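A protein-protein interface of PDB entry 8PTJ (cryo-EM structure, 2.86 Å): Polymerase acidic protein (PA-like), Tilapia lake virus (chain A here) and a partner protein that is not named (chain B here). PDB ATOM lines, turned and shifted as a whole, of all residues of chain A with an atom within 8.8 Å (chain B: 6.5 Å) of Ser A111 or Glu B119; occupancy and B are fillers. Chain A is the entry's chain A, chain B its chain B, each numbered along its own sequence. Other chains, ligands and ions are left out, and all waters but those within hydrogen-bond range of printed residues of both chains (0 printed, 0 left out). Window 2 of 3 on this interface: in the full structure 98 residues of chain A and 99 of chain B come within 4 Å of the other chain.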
ATOM      1  N   HIS A 108      10.172 -16.312  -1.823  1.00  0.00           N
ATOM      2  CA  HIS A 108       9.128 -17.155  -2.389  1.00  0.00           C
ATOM      3  C   HIS A 108       9.316 -18.603  -1.959  1.00  0.00           C
ATOM      4  O   HIS A 108      10.426 -19.140  -1.992  1.00  0.00           O
ATOM      5  CB  HIS A 108       9.139 -17.054  -3.913  1.00  0.00           C
ATOM      6  CG  HIS A 108       8.037 -17.817  -4.576  1.00  0.00           C
ATOM      7  ND1 HIS A 108       6.823 -17.245  -4.893  1.00  0.00           N
ATOM      8  CD2 HIS A 108       7.962 -19.105  -4.986  1.00  0.00           C
ATOM      9  CE1 HIS A 108       6.050 -18.148  -5.467  1.00  0.00           C
ATOM     10  NE2 HIS A 108       6.717 -19.285  -5.536  1.00  0.00           N
ATOM     11  N   LYS A 109       8.219 -19.236  -1.554  1.00  0.00           N
ATOM     12  CA  LYS A 109       8.216 -20.623  -1.111  1.00  0.00           C
ATOM     13  C   LYS A 109       7.554 -21.478  -2.183  1.00  0.00           C
ATOM     14  O   LYS A 109       6.389 -21.253  -2.530  1.00  0.00           O
ATOM     15  CB  LYS A 109       7.484 -20.766   0.223  1.00  0.00           C
ATOM     16  CG  LYS A 109       7.444 -22.185   0.762  1.00  0.00           C
ATOM     17  CD  LYS A 109       6.800 -22.236   2.138  1.00  0.00           C
ATOM     18  CE  LYS A 109       6.718 -23.661   2.661  1.00  0.00           C
ATOM     19  NZ  LYS A 109       6.082 -23.727   4.005  1.00  0.00           N
ATOM     20  N   ALA A 110       8.292 -22.453  -2.701  1.00  0.00           N
ATOM     21  CA  ALA A 110       7.791 -23.327  -3.748  1.00  0.00           C
ATOM     22  C   ALA A 110       7.001 -24.488  -3.149  1.00  0.00           C
ATOM     23  O   ALA A 110       7.065 -24.770  -1.951  1.00  0.00           O
ATOM     24  CB  ALA A 110       8.945 -23.851  -4.601  1.00  0.00           C
ATOM     25  N   SER A 111       6.242 -25.168  -4.011  1.00  0.00           N
ATOM     26  CA  SER A 111       5.425 -26.290  -3.569  1.00  0.00           C
ATOM     27  C   SER A 111       6.262 -27.473  -3.100  1.00  0.00           C
ATOM     28  O   SER A 111       5.750 -28.322  -2.363  1.00  0.00           O
ATOM     29  CB  SER A 111       4.496 -26.736  -4.698  1.00  0.00           C
ATOM     30  OG  SER A 111       5.208 -27.459  -5.686  1.00  0.00           O
ATOM     31  N   TYR A 112       7.526 -27.548  -3.506  1.00  0.00           N
ATOM     32  CA  TYR A 112       8.405 -28.652  -3.147  1.00  0.00           C
ATOM     33  C   TYR A 112       9.354 -28.298  -2.010  1.00  0.00           C
ATOM     34  O   TYR A 112      10.300 -29.047  -1.749  1.00  0.00           O
ATOM     35  CB  TYR A 112       9.207 -29.107  -4.368  1.00  0.00           C
ATOM     36  CG  TYR A 112       9.845 -27.977  -5.141  1.00  0.00           C
ATOM     37  CD1 TYR A 112      10.983 -27.339  -4.666  1.00  0.00           C
ATOM     38  CD2 TYR A 112       9.308 -27.544  -6.345  1.00  0.00           C
ATOM     39  CE1 TYR A 112      11.566 -26.306  -5.367  1.00  0.00           C
ATOM     40  CE2 TYR A 112       9.885 -26.511  -7.052  1.00  0.00           C
ATOM     41  CZ  TYR A 112      11.014 -25.897  -6.560  1.00  0.00           C
ATOM     42  OH  TYR A 112      11.590 -24.866  -7.263  1.00  0.00           O
ATOM     43  N   ASP A 113       9.124 -27.174  -1.328  1.00  0.00           N
ATOM     44  CA  ASP A 113      10.018 -26.766  -0.248  1.00  0.00           C
ATOM     45  C   ASP A 113      10.038 -27.803   0.868  1.00  0.00           C
ATOM     46  O   ASP A 113      11.107 -28.172   1.370  1.00  0.00           O
ATOM     47  CB  ASP A 113       9.585 -25.403   0.292  1.00  0.00           C
ATOM     48  CG  ASP A 113      10.651 -24.747   1.144  1.00  0.00           C
ATOM     49  OD1 ASP A 113      10.968 -25.289   2.224  1.00  0.00           O
ATOM     50  OD2 ASP A 113      11.175 -23.690   0.735  1.00  0.00           O
ATOM     51  N   ALA A 114       8.862 -28.289   1.267  1.00  0.00           N
ATOM     52  CA  ALA A 114       8.793 -29.245   2.367  1.00  0.00           C
ATOM     53  C   ALA A 114       9.493 -30.549   2.013  1.00  0.00           C
ATOM     54  O   ALA A 114      10.195 -31.132   2.846  1.00  0.00           O
ATOM     55  CB  ALA A 114       7.336 -29.505   2.744  1.00  0.00           C
ATOM     56  N   GLU A 115       9.307 -31.032   0.782  1.00  0.00           N
ATOM     57  CA  GLU A 115       9.942 -32.282   0.380  1.00  0.00           C
ATOM     58  C   GLU A 115      11.460 -32.162   0.409  1.00  0.00           C
ATOM     59  O   GLU A 115      12.154 -33.058   0.904  1.00  0.00           O
ATOM     60  CB  GLU A 115       9.462 -32.685  -1.015  1.00  0.00           C
ATOM     61  CG  GLU A 115      10.395 -33.643  -1.736  1.00  0.00           C
ATOM     62  CD  GLU A 115       9.707 -34.384  -2.863  1.00  0.00           C
ATOM     63  OE1 GLU A 115       8.698 -33.868  -3.386  1.00  0.00           O
ATOM     64  OE2 GLU A 115      10.176 -35.484  -3.225  1.00  0.00           O
ATOM     65  N   LEU A 116      11.996 -31.060  -0.117  1.00  0.00           N
ATOM     66  CA  LEU A 116      13.440 -30.864  -0.091  1.00  0.00           C
ATOM     67  C   LEU A 116      13.946 -30.715   1.336  1.00  0.00           C
ATOM     68  O   LEU A 116      15.041 -31.183   1.663  1.00  0.00           O
ATOM     69  CB  LEU A 116      13.820 -29.642  -0.927  1.00  0.00           C
ATOM     70  CG  LEU A 116      13.569 -29.760  -2.431  1.00  0.00           C
ATOM     71  CD1 LEU A 116      13.968 -28.475  -3.131  1.00  0.00           C
ATOM     72  CD2 LEU A 116      14.313 -30.945  -3.023  1.00  0.00           C
ATOM     73  N   LEU B 116      10.686 -21.703  -9.743  1.00  0.00           N
ATOM     74  CA  LEU B 116       9.982 -21.424  -8.497  1.00  0.00           C
ATOM     75  C   LEU B 116       8.471 -21.586  -8.612  1.00  0.00           C
ATOM     76  O   LEU B 116       7.794 -21.658  -7.581  1.00  0.00           O
ATOM     77  CB  LEU B 116      10.301 -20.006  -8.022  1.00  0.00           C
ATOM     78  CG  LEU B 116      11.666 -19.800  -7.368  1.00  0.00           C
ATOM     79  CD1 LEU B 116      11.958 -18.318  -7.218  1.00  0.00           C
ATOM     80  CD2 LEU B 116      11.732 -20.495  -6.019  1.00  0.00           C
ATOM     81  N   THR B 117       7.925 -21.643  -9.828  1.00  0.00           N
ATOM     82  CA  THR B 117       6.479 -21.648 -10.008  1.00  0.00           C
ATOM     83  C   THR B 117       5.880 -23.035 -10.203  1.00  0.00           C
ATOM     84  O   THR B 117       4.658 -23.179 -10.086  1.00  0.00           O
ATOM     85  CB  THR B 117       6.094 -20.779 -11.211  1.00  0.00           C
ATOM     86  OG1 THR B 117       7.038 -20.976 -12.268  1.00  0.00           O
ATOM     87  CG2 THR B 117       6.068 -19.308 -10.820  1.00  0.00           C
ATOM     88  N   VAL B 118       6.691 -24.055 -10.497  1.00  0.00           N
ATOM     89  CA  VAL B 118       6.125 -25.381 -10.726  1.00  0.00           C
ATOM     90  C   VAL B 118       5.429 -25.877  -9.460  1.00  0.00           C
ATOM     91  O   VAL B 118       5.669 -25.392  -8.347  1.00  0.00           O
ATOM     92  CB  VAL B 118       7.194 -26.387 -11.182  1.00  0.00           C
ATOM     93  CG1 VAL B 118       7.731 -26.013 -12.550  1.00  0.00           C
ATOM     94  CG2 VAL B 118       8.321 -26.478 -10.164  1.00  0.00           C
ATOM     95  N   GLU B 119       4.552 -26.862  -9.642  1.00  0.00           N
ATOM     96  CA  GLU B 119       3.831 -27.490  -8.542  1.00  0.00           C
ATOM     97  C   GLU B 119       4.255 -28.937  -8.328  1.00  0.00           C
ATOM     98  O   GLU B 119       3.559 -29.681  -7.632  1.00  0.00           O
ATOM     99  CB  GLU B 119       2.313 -27.417  -8.760  1.00  0.00           C
ATOM    100  CG  GLU B 119       1.790 -27.993 -10.073  1.00  0.00           C
ATOM    101  CD  GLU B 119       2.150 -27.150 -11.278  1.00  0.00           C
ATOM    102  OE1 GLU B 119       1.226 -26.703 -11.989  1.00  0.00           O
ATOM    103  OE2 GLU B 119       3.354 -26.917 -11.506  1.00  0.00           O
ATOM    104  N   SER B 120       5.374 -29.353  -8.913  1.00  0.00           N
ATOM    105  CA  SER B 120       5.914 -30.683  -8.680  1.00  0.00           C
ATOM    106  C   SER B 120       7.364 -30.701  -9.136  1.00  0.00           C
ATOM    107  O   SER B 120       7.759 -29.938 -10.021  1.00  0.00           O
ATOM    108  CB  SER B 120       5.106 -31.756  -9.416  1.00  0.00           C
ATOM    109  OG  SER B 120       5.490 -33.054  -9.003  1.00  0.00           O
ATOM    110  N   LEU B 121       8.155 -31.582  -8.521  1.00  0.00           N
ATOM    111  CA  LEU B 121       9.556 -31.707  -8.900  1.00  0.00           C
ATOM    112  C   LEU B 121       9.730 -32.429 -10.228  1.00  0.00           C
ATOM    113  O   LEU B 121      10.793 -32.312 -10.847  1.00  0.00           O
ATOM    114  CB  LEU B 121      10.332 -32.446  -7.808  1.00  0.00           C
ATOM    115  CG  LEU B 121      10.774 -31.606  -6.608  1.00  0.00           C
ATOM    116  CD1 LEU B 121      11.254 -32.501  -5.478  1.00  0.00           C
ATOM    117  CD2 LEU B 121      11.862 -30.624  -7.006  1.00  0.00           C
ATOM    118  N   GLU B 123       7.610 -32.030 -12.915  1.00  0.00           N
ATOM    119  CA  GLU B 123       7.037 -31.292 -14.030  1.00  0.00           C
ATOM    120  C   GLU B 123       8.133 -30.803 -14.970  1.00  0.00           C
ATOM    121  O   GLU B 123       9.248 -30.484 -14.551  1.00  0.00           O
ATOM    122  CB  GLU B 123       6.213 -30.109 -13.524  1.00  0.00           C
ATOM    123  CG  GLU B 123       5.999 -29.017 -14.562  1.00  0.00           C
ATOM    124  CD  GLU B 123       4.903 -28.051 -14.175  1.00  0.00           C
ATOM    125  OE1 GLU B 123       4.099 -28.396 -13.286  1.00  0.00           O
ATOM    126  OE2 GLU B 123       4.844 -26.948 -14.759  1.00  0.00           O
ATOM    127  N   SER B 237      12.627 -21.001  -0.873  1.00  0.00           N
ATOM    128  CA  SER B 237      12.979 -22.264  -1.511  1.00  0.00           C
ATOM    129  C   SER B 237      14.317 -22.206  -2.236  1.00  0.00           C
ATOM    130  O   SER B 237      14.931 -23.255  -2.451  1.00  0.00           O
ATOM    131  CB  SER B 237      11.884 -22.678  -2.491  1.00  0.00           C
ATOM    132  OG  SER B 237      10.837 -23.356  -1.823  1.00  0.00           O
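The backbone carbonyl oxygen (O) of Glu B119 lies close to the side-chain hydroxyl (OG) of Ser A111. The backbone NH (N) of Ser B237 sits at hydrogen-bond distance from the backbone carbonyl oxygen (O) of His A108, at 3.1 Å. The side-chain carboxylate (OD2) of Asp A113 sits at hydrogen-bond distance from the side-chain hydroxyl (OG) of Ser B237 (2.6 Å). OG of Ser A111 lies within hydrogen-bond range of O of Val B118. NE2 of His A108 sits at hydrogen-bond distance from O of Leu B116 (3.3 Å). The side-chain hydroxyl (OG) of Ser B237 sits at hydrogen-bond distance from the backbone NH (N) of Ala A110, 2.8 Å away.
The side-chain carboxylate (OE2) of Glu B119 lies close to the side-chain carboxylate (OE1) of Glu B123, 2.4 Å away.
Among the printed residues, pairs that only touch across the chains: Tyr A112 with Val B118 (3.5 Å), Glu A115 with Leu B121 (3.6 Å), Tyr A112 with Leu B121 (3.7 Å), Ser A111 with Ser B120 (3.7 Å), Lys A109 with Ser B237 (3.8 Å), Ala A110 with Leu B116 (3.9 Å) and Tyr A112 with Leu B116 (3.99 Å).
Of chain B, only Val B118 (3.4 Å), Glu B119 (3.2 Å) and Ser B120 (3.7 Å) come within 4 Å of Ser A111. Printed residues of chain A within 4 Å of Glu B119: Ser A111 (3.2 Å). Val B118 touches two residues of chain A. Of chain A, only Ser A111 comes within 4 Å of Ser B120. Of the printed residues of chain B, Ala A110 touches Leu B116 and Ser B237. Printed residues of chain B within 4 Å of Glu A115: Leu B121. Ala A114 touches none of the printed residues of chain B. Glu B123 touches none of the printed residues of chain A. The nearest residue of chain B that does not touch Ser A111 is Leu B116 (5.2 Å).
Among the printed residues, 13 pairs touch across the chains.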
